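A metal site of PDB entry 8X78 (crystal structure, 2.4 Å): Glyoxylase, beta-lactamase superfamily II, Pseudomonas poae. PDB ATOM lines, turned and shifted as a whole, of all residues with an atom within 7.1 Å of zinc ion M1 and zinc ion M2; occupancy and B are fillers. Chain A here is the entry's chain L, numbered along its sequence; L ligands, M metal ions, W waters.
ND1 of His 263 lies close to SD of Met 46, 3.6 Å away.
The backbone NH (N) of His 263 lies within hydrogen-bond range of the backbone carbonyl oxygen (O) of Tyr 220, at 3.1 Å.
O of Asp 111 sits at hydrogen-bond distance from OH of Tyr 20 (3.1 Å).
O of His 196 sits at hydrogen-bond distance from N of Gln 235 (3.0 Å).
NE2 of His 109 sits at hydrogen-bond distance from OE1 of Gln 235, 2.9 Å away.
OD2 of Asp 217 lies close to NE2 of His 107 (2.6 Å).
A ring nitrogen (ND1) of His 109 sits close to a ring nitrogen (NE2) of His 107.
A ring nitrogen (ND1) of His 112 lies within hydrogen-bond range of the side-chain carboxylate (OD2) of Asp 66 (2.6 Å).
Within 4 Å of zinc ion M1: Asp 111, His 112, Asp 217 and His 263.
The nearest printed residue that does not touch zinc ion M1 is His 107 (4.2 Å).
Residues that only touch zinc ion M2: Tyr 220.
Zinc ion M1 is bound by water W1 (1.9 Å), a ring nitrogen (NE2) of His 112 (2.2 Å), a ring nitrogen (NE2) of His 263 (2.3 Å), the side-chain carboxylate of Asp 217 (2.3 Å) and the side-chain carboxylate of Asp 111 (2.6 Å).
Zinc ion M1 has five donor atoms within binding distance.
Slightly farther from zinc ion M1 lies O2 of the ligand (2.8 Å).
Zinc ion M2 is bound by a ring nitrogen (ND1) of His 109.
Zinc ion M2 is bound by OD2 of Asp 217, 2.3 Å away.
NE2 of His 196 is bound to zinc ion M2.
Slightly farther from zinc ion M2 lies NE2 of His 107 (2.6 Å).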
ATOM      1  N   TYR A  20      -0.781   2.326  31.425  1.00  0.00           N
ATOM      2  CA  TYR A  20      -0.613   1.492  32.616  1.00  0.00           C
ATOM      3  C   TYR A  20       0.134   2.195  33.722  1.00  0.00           C
ATOM      4  O   TYR A  20       0.225   1.642  34.835  1.00  0.00           O
ATOM      5  CB  TYR A  20       0.123   0.184  32.263  1.00  0.00           C
ATOM      6  CG  TYR A  20       1.573   0.379  31.871  1.00  0.00           C
ATOM      7  CD1 TYR A  20       1.929   0.714  30.554  1.00  0.00           C
ATOM      8  CD2 TYR A  20       2.603   0.226  32.810  1.00  0.00           C
ATOM      9  CE1 TYR A  20       3.266   0.884  30.193  1.00  0.00           C
ATOM     10  CE2 TYR A  20       3.932   0.389  32.447  1.00  0.00           C
ATOM     11  CZ  TYR A  20       4.256   0.725  31.142  1.00  0.00           C
ATOM     12  OH  TYR A  20       5.577   0.895  30.787  1.00  0.00           O
ATOM     13  N   PHE A  30      11.624  14.294  26.275  1.00  0.00           N
ATOM     14  CA  PHE A  30      10.825  13.705  25.219  1.00  0.00           C
ATOM     15  C   PHE A  30      10.733  14.594  23.978  1.00  0.00           C
ATOM     16  O   PHE A  30      10.582  14.080  22.871  1.00  0.00           O
ATOM     17  CB  PHE A  30       9.406  13.428  25.732  1.00  0.00           C
ATOM     18  CG  PHE A  30       9.321  12.359  26.808  1.00  0.00           C
ATOM     19  CD1 PHE A  30       9.835  11.085  26.582  1.00  0.00           C
ATOM     20  CD2 PHE A  30       8.671  12.619  28.015  1.00  0.00           C
ATOM     21  CE1 PHE A  30       9.732  10.098  27.552  1.00  0.00           C
ATOM     22  CE2 PHE A  30       8.570  11.639  29.006  1.00  0.00           C
ATOM     23  CZ  PHE A  30       9.100  10.378  28.774  1.00  0.00           C
ATOM     24  N   MET A  46       2.721   6.115  30.256  1.00  0.00           N
ATOM     25  CA  MET A  46       3.405   4.872  29.920  1.00  0.00           C
ATOM     26  C   MET A  46       2.342   3.970  29.295  1.00  0.00           C
ATOM     27  O   MET A  46       1.279   3.754  29.885  1.00  0.00           O
ATOM     28  CB  MET A  46       4.052   4.244  31.161  1.00  0.00           C
ATOM     29  CG  MET A  46       4.856   5.272  31.978  1.00  0.00           C
ATOM     30  SD  MET A  46       6.400   5.800  31.183  1.00  0.00           S
ATOM     31  CE  MET A  46       7.192   4.194  31.036  1.00  0.00           C
ATOM     32  N   ASP A  66       4.433  -3.917  22.785  1.00  0.00           N
ATOM     33  CA  ASP A  66       5.032  -3.603  24.072  1.00  0.00           C
ATOM     34  C   ASP A  66       4.106  -4.038  25.202  1.00  0.00           C
ATOM     35  O   ASP A  66       2.915  -4.325  24.999  1.00  0.00           O
ATOM     36  CB  ASP A  66       5.364  -2.117  24.137  1.00  0.00           C
ATOM     37  CG  ASP A  66       6.424  -1.705  23.105  1.00  0.00           C
ATOM     38  OD1 ASP A  66       7.204  -2.587  22.668  1.00  0.00           O
ATOM     39  OD2 ASP A  66       6.447  -0.518  22.687  1.00  0.00           O
ATOM     40  N   THR A 106       8.857  -3.073  20.339  1.00  0.00           N
ATOM     41  CA  THR A 106       9.486  -1.979  19.587  1.00  0.00           C
ATOM     42  C   THR A 106      10.979  -1.905  19.878  1.00  0.00           C
ATOM     43  O   THR A 106      11.779  -1.712  18.958  1.00  0.00           O
ATOM     44  CB  THR A 106       8.801  -0.644  19.913  1.00  0.00           C
ATOM     45  OG1 THR A 106       8.798  -0.416  21.325  1.00  0.00           O
ATOM     46  CG2 THR A 106       7.379  -0.609  19.405  1.00  0.00           C
ATOM     47  N   HIS A 107      11.378  -2.085  21.143  1.00  0.00           N
ATOM     48  CA  HIS A 107      12.778  -2.012  21.564  1.00  0.00           C
ATOM     49  C   HIS A 107      12.890  -2.546  22.984  1.00  0.00           C
ATOM     50  O   HIS A 107      11.888  -2.753  23.672  1.00  0.00           O
ATOM     51  CB  HIS A 107      13.341  -0.579  21.442  1.00  0.00           C
ATOM     52  CG  HIS A 107      12.700   0.425  22.365  1.00  0.00           C
ATOM     53  ND1 HIS A 107      11.349   0.669  22.387  1.00  0.00           N
ATOM     54  CD2 HIS A 107      13.258   1.312  23.226  1.00  0.00           C
ATOM     55  CE1 HIS A 107      11.084   1.653  23.245  1.00  0.00           C
ATOM     56  NE2 HIS A 107      12.230   2.052  23.770  1.00  0.00           N
ATOM     57  N   MET A 108      14.123  -2.792  23.426  1.00  0.00           N
ATOM     58  CA  MET A 108      14.339  -3.516  24.673  1.00  0.00           C
ATOM     59  C   MET A 108      14.540  -2.597  25.884  1.00  0.00           C
ATOM     60  O   MET A 108      15.044  -3.057  26.924  1.00  0.00           O
ATOM     61  CB  MET A 108      15.522  -4.479  24.520  1.00  0.00           C
ATOM     62  CG  MET A 108      15.129  -5.736  23.717  1.00  0.00           C
ATOM     63  SD  MET A 108      16.484  -6.862  23.358  1.00  0.00           S
ATOM     64  CE  MET A 108      16.817  -7.470  25.033  1.00  0.00           C
ATOM     65  N   HIS A 109      14.116  -1.338  25.803  1.00  0.00           N
ATOM     66  CA  HIS A 109      14.052  -0.543  27.023  1.00  0.00           C
ATOM     67  C   HIS A 109      13.103  -1.206  28.008  1.00  0.00           C
ATOM     68  O   HIS A 109      12.113  -1.829  27.625  1.00  0.00           O
ATOM     69  CB  HIS A 109      13.592   0.872  26.696  1.00  0.00           C
ATOM     70  CG  HIS A 109      14.681   1.758  26.158  1.00  0.00           C
ATOM     71  ND1 HIS A 109      14.430   2.995  25.594  1.00  0.00           N
ATOM     72  CD2 HIS A 109      16.024   1.579  26.093  1.00  0.00           C
ATOM     73  CE1 HIS A 109      15.573   3.548  25.230  1.00  0.00           C
ATOM     74  NE2 HIS A 109      16.550   2.701  25.509  1.00  0.00           N
ATOM     75  N   PHE A 110      13.405  -1.058  29.304  1.00  0.00           N
ATOM     76  CA  PHE A 110      12.712  -1.804  30.357  1.00  0.00           C
ATOM     77  C   PHE A 110      11.209  -1.608  30.286  1.00  0.00           C
ATOM     78  O   PHE A 110      10.432  -2.534  30.556  1.00  0.00           O
ATOM     79  CB  PHE A 110      13.221  -1.390  31.725  1.00  0.00           C
ATOM     80  CG  PHE A 110      12.753  -0.031  32.151  1.00  0.00           C
ATOM     81  CD1 PHE A 110      13.330   1.108  31.624  1.00  0.00           C
ATOM     82  CD2 PHE A 110      11.736   0.102  33.091  1.00  0.00           C
ATOM     83  CE1 PHE A 110      12.905   2.360  32.008  1.00  0.00           C
ATOM     84  CE2 PHE A 110      11.308   1.354  33.485  1.00  0.00           C
ATOM     85  CZ  PHE A 110      11.895   2.486  32.950  1.00  0.00           C
ATOM     86  N   ASP A 111      10.772  -0.399  29.972  1.00  0.00           N
ATOM     87  CA  ASP A 111       9.356  -0.103  29.999  1.00  0.00           C
ATOM     88  C   ASP A 111       8.626  -0.568  28.736  1.00  0.00           C
ATOM     89  O   ASP A 111       7.438  -0.247  28.576  1.00  0.00           O
ATOM     90  CB  ASP A 111       9.133   1.394  30.194  1.00  0.00           C
ATOM     91  CG  ASP A 111       9.773   2.221  29.107  1.00  0.00           C
ATOM     92  OD1 ASP A 111      10.946   1.959  28.736  1.00  0.00           O
ATOM     93  OD2 ASP A 111       9.098   3.175  28.652  1.00  0.00           O
ATOM     94  N   HIS A 112       9.294  -1.290  27.815  1.00  0.00           N
ATOM     95  CA  HIS A 112       8.584  -1.881  26.701  1.00  0.00           C
ATOM     96  C   HIS A 112       8.657  -3.397  26.652  1.00  0.00           C
ATOM     97  O   HIS A 112       7.757  -4.010  26.076  1.00  0.00           O
ATOM     98  CB  HIS A 112       9.096  -1.269  25.400  1.00  0.00           C
ATOM     99  CG  HIS A 112       8.827   0.196  25.323  1.00  0.00           C
ATOM    100  ND1 HIS A 112       7.725   0.698  24.661  1.00  0.00           N
ATOM    101  CD2 HIS A 112       9.428   1.252  25.919  1.00  0.00           C
ATOM    102  CE1 HIS A 112       7.686   2.011  24.820  1.00  0.00           C
ATOM    103  NE2 HIS A 112       8.710   2.366  25.569  1.00  0.00           N
ATOM    104  N   SER A 156      17.733   3.337  30.752  1.00  0.00           N
ATOM    105  CA  SER A 156      16.470   2.734  30.327  1.00  0.00           C
ATOM    106  C   SER A 156      16.598   1.257  30.055  1.00  0.00           C
ATOM    107  O   SER A 156      15.690   0.673  29.457  1.00  0.00           O
ATOM    108  CB  SER A 156      15.943   3.422  29.057  1.00  0.00           C
ATOM    109  OG  SER A 156      15.591   4.774  29.298  1.00  0.00           O
ATOM    110  N   HIS A 196      15.942   5.079  17.577  1.00  0.00           N
ATOM    111  CA  HIS A 196      15.886   5.230  19.035  1.00  0.00           C
ATOM    112  C   HIS A 196      16.900   4.334  19.739  1.00  0.00           C
ATOM    113  O   HIS A 196      17.510   4.741  20.730  1.00  0.00           O
ATOM    114  CB  HIS A 196      14.488   4.937  19.574  1.00  0.00           C
ATOM    115  CG  HIS A 196      14.359   5.176  21.046  1.00  0.00           C
ATOM    116  ND1 HIS A 196      14.432   6.431  21.596  1.00  0.00           N
ATOM    117  CD2 HIS A 196      14.225   4.309  22.071  1.00  0.00           C
ATOM    118  CE1 HIS A 196      14.299   6.335  22.916  1.00  0.00           C
ATOM    119  NE2 HIS A 196      14.171   5.057  23.220  1.00  0.00           N
ATOM    120  N   THR A 197      17.070   3.103  19.244  1.00  0.00           N
ATOM    121  CA  THR A 197      18.016   2.150  19.783  1.00  0.00           C
ATOM    122  C   THR A 197      18.555   1.341  18.619  1.00  0.00           C
ATOM    123  O   THR A 197      18.022   1.423  17.512  1.00  0.00           O
ATOM    124  CB  THR A 197      17.381   1.197  20.827  1.00  0.00           C
ATOM    125  OG1 THR A 197      16.301   0.471  20.221  1.00  0.00           O
ATOM    126  CG2 THR A 197      16.857   1.945  22.087  1.00  0.00           C
ATOM    127  N   SER A 200      15.559  -0.616  16.985  1.00  0.00           N
ATOM    128  CA  SER A 200      14.168  -0.188  17.083  1.00  0.00           C
ATOM    129  C   SER A 200      13.378  -0.631  15.856  1.00  0.00           C
ATOM    130  O   SER A 200      13.887  -0.618  14.730  1.00  0.00           O
ATOM    131  CB  SER A 200      14.092   1.333  17.225  1.00  0.00           C
ATOM    132  OG  SER A 200      14.270   1.719  18.565  1.00  0.00           O
ATOM    133  N   GLY A 216       6.560   3.294  18.778  1.00  0.00           N
ATOM    134  CA  GLY A 216       7.508   3.083  19.849  1.00  0.00           C
ATOM    135  C   GLY A 216       8.096   4.392  20.291  1.00  0.00           C
ATOM    136  O   GLY A 216       7.434   5.418  20.234  1.00  0.00           O
ATOM    137  N   ASP A 217       9.353   4.379  20.713  1.00  0.00           N
ATOM    138  CA  ASP A 217       9.993   5.593  21.189  1.00  0.00           C
ATOM    139  C   ASP A 217      10.673   6.376  20.112  1.00  0.00           C
ATOM    140  O   ASP A 217      11.228   7.429  20.385  1.00  0.00           O
ATOM    141  CB  ASP A 217      10.960   5.260  22.304  1.00  0.00           C
ATOM    142  CG  ASP A 217      10.244   4.919  23.565  1.00  0.00           C
ATOM    143  OD1 ASP A 217       9.087   5.357  23.747  1.00  0.00           O
ATOM    144  OD2 ASP A 217      10.821   4.201  24.371  1.00  0.00           O
ATOM    145  N   ILE A 218      10.713   5.858  18.891  1.00  0.00           N
ATOM    146  CA  ILE A 218      11.190   6.671  17.781  1.00  0.00           C
ATOM    147  C   ILE A 218      10.466   8.003  17.765  1.00  0.00           C
ATOM    148  O   ILE A 218      11.069   9.061  17.565  1.00  0.00           O
ATOM    149  CB  ILE A 218      11.003   5.939  16.443  1.00  0.00           C
ATOM    150  CG1 ILE A 218      11.767   4.613  16.449  1.00  0.00           C
ATOM    151  CG2 ILE A 218      11.490   6.845  15.286  1.00  0.00           C
ATOM    152  CD1 ILE A 218      11.413   3.755  15.271  1.00  0.00           C
ATOM    153  N   TYR A 220       8.579   9.875  20.501  1.00  0.00           N
ATOM    154  CA  TYR A 220       8.102  10.066  21.868  1.00  0.00           C
ATOM    155  C   TYR A 220       6.798  10.840  21.892  1.00  0.00           C
ATOM    156  O   TYR A 220       5.824  10.448  22.554  1.00  0.00           O
ATOM    157  CB  TYR A 220       9.152  10.814  22.704  1.00  0.00           C
ATOM    158  CG  TYR A 220      10.227   9.994  23.384  1.00  0.00           C
ATOM    159  CD1 TYR A 220       9.978   8.716  23.863  1.00  0.00           C
ATOM    160  CD2 TYR A 220      11.486  10.527  23.568  1.00  0.00           C
ATOM    161  CE1 TYR A 220      10.967   7.986  24.500  1.00  0.00           C
ATOM    162  CE2 TYR A 220      12.486   9.803  24.188  1.00  0.00           C
ATOM    163  CZ  TYR A 220      12.225   8.540  24.664  1.00  0.00           C
ATOM    164  OH  TYR A 220      13.237   7.844  25.298  1.00  0.00           O
ATOM    165  N   TYR A 233      16.702  12.995  24.806  1.00  0.00           N
ATOM    166  CA  TYR A 233      17.201  11.702  25.228  1.00  0.00           C
ATOM    167  C   TYR A 233      16.827  10.665  24.176  1.00  0.00           C
ATOM    168  O   TYR A 233      15.641  10.516  23.842  1.00  0.00           O
ATOM    169  CB  TYR A 233      16.617  11.283  26.586  1.00  0.00           C
ATOM    170  CG  TYR A 233      16.947   9.857  26.960  1.00  0.00           C
ATOM    171  CD1 TYR A 233      18.158   9.544  27.551  1.00  0.00           C
ATOM    172  CD2 TYR A 233      16.047   8.825  26.687  1.00  0.00           C
ATOM    173  CE1 TYR A 233      18.473   8.233  27.892  1.00  0.00           C
ATOM    174  CE2 TYR A 233      16.359   7.485  27.037  1.00  0.00           C
ATOM    175  CZ  TYR A 233      17.579   7.221  27.632  1.00  0.00           C
ATOM    176  OH  TYR A 233      17.922   5.937  27.981  1.00  0.00           O
ATOM    177  N   HIS A 234      17.831   9.975  23.647  1.00  0.00           N
ATOM    178  CA  HIS A 234      17.635   8.803  22.806  1.00  0.00           C
ATOM    179  C   HIS A 234      18.969   8.079  22.760  1.00  0.00           C
ATOM    180  O   HIS A 234      19.994   8.628  23.161  1.00  0.00           O
ATOM    181  CB  HIS A 234      17.140   9.168  21.415  1.00  0.00           C
ATOM    182  CG  HIS A 234      18.139   9.944  20.622  1.00  0.00           C
ATOM    183  ND1 HIS A 234      19.237   9.365  20.038  1.00  0.00           N
ATOM    184  CD2 HIS A 234      18.194  11.261  20.298  1.00  0.00           C
ATOM    185  CE1 HIS A 234      19.942  10.283  19.406  1.00  0.00           C
ATOM    186  NE2 HIS A 234      19.328  11.450  19.551  1.00  0.00           N
ATOM    187  N   GLN A 235      18.963   6.833  22.290  1.00  0.00           N
ATOM    188  CA  GLN A 235      20.207   6.068  22.302  1.00  0.00           C
ATOM    189  C   GLN A 235      20.578   5.534  20.911  1.00  0.00           C
ATOM    190  O   GLN A 235      21.204   4.487  20.771  1.00  0.00           O
ATOM    191  CB  GLN A 235      20.129   4.957  23.348  1.00  0.00           C
ATOM    192  CG  GLN A 235      19.825   5.524  24.737  1.00  0.00           C
ATOM    193  CD  GLN A 235      20.056   4.512  25.848  1.00  0.00           C
ATOM    194  OE1 GLN A 235      19.315   3.541  25.951  1.00  0.00           O
ATOM    195  NE2 GLN A 235      21.090   4.724  26.650  1.00  0.00           N
ATOM    196  N   GLY A 262       5.001   7.112  21.783  1.00  0.00           N
ATOM    197  CA  GLY A 262       5.320   6.329  22.964  1.00  0.00           C
ATOM    198  C   GLY A 262       4.861   6.868  24.300  1.00  0.00           C
ATOM    199  O   GLY A 262       4.441   6.095  25.177  1.00  0.00           O
ATOM    200  N   HIS A 263       4.948   8.190  24.482  1.00  0.00           N
ATOM    201  CA  HIS A 263       4.878   8.813  25.801  1.00  0.00           C
ATOM    202  C   HIS A 263       4.276  10.213  25.726  1.00  0.00           C
ATOM    203  O   HIS A 263       4.787  11.152  26.337  1.00  0.00           O
ATOM    204  CB  HIS A 263       6.279   8.924  26.389  1.00  0.00           C
ATOM    205  CG  HIS A 263       6.900   7.609  26.709  1.00  0.00           C
ATOM    206  ND1 HIS A 263       6.472   6.810  27.750  1.00  0.00           N
ATOM    207  CD2 HIS A 263       7.857   6.903  26.054  1.00  0.00           C
ATOM    208  CE1 HIS A 263       7.191   5.705  27.768  1.00  0.00           C
ATOM    209  NE2 HIS A 263       8.022   5.723  26.729  1.00  0.00           N
HETATM  210  C1  LIG L   1      12.476   5.911  29.523  1.00  0.00           C
HETATM  211  O1  LIG L   1      13.194   6.640  30.497  1.00  0.00           O
HETATM  212  C2  LIG L   1      11.239   6.739  29.037  1.00  0.00           C
HETATM  213  O2  LIG L   1      10.872   6.317  27.739  1.00  0.00           O
HETATM  214  C3  LIG L   1      10.137   6.531  30.124  1.00  0.00           C
HETATM  215  O3  LIG L   1      10.549   7.232  31.274  1.00  0.00           O
HETATM  216 ZN    ZN M   1       9.670   4.203  26.360  1.00  0.00          ZN
HETATM  217 ZN    ZN M   2      13.025   4.228  25.040  1.00  0.00          ZN
HETATM  218  O   HOH W   1      11.299   3.861  27.354  1.00  0.00           O
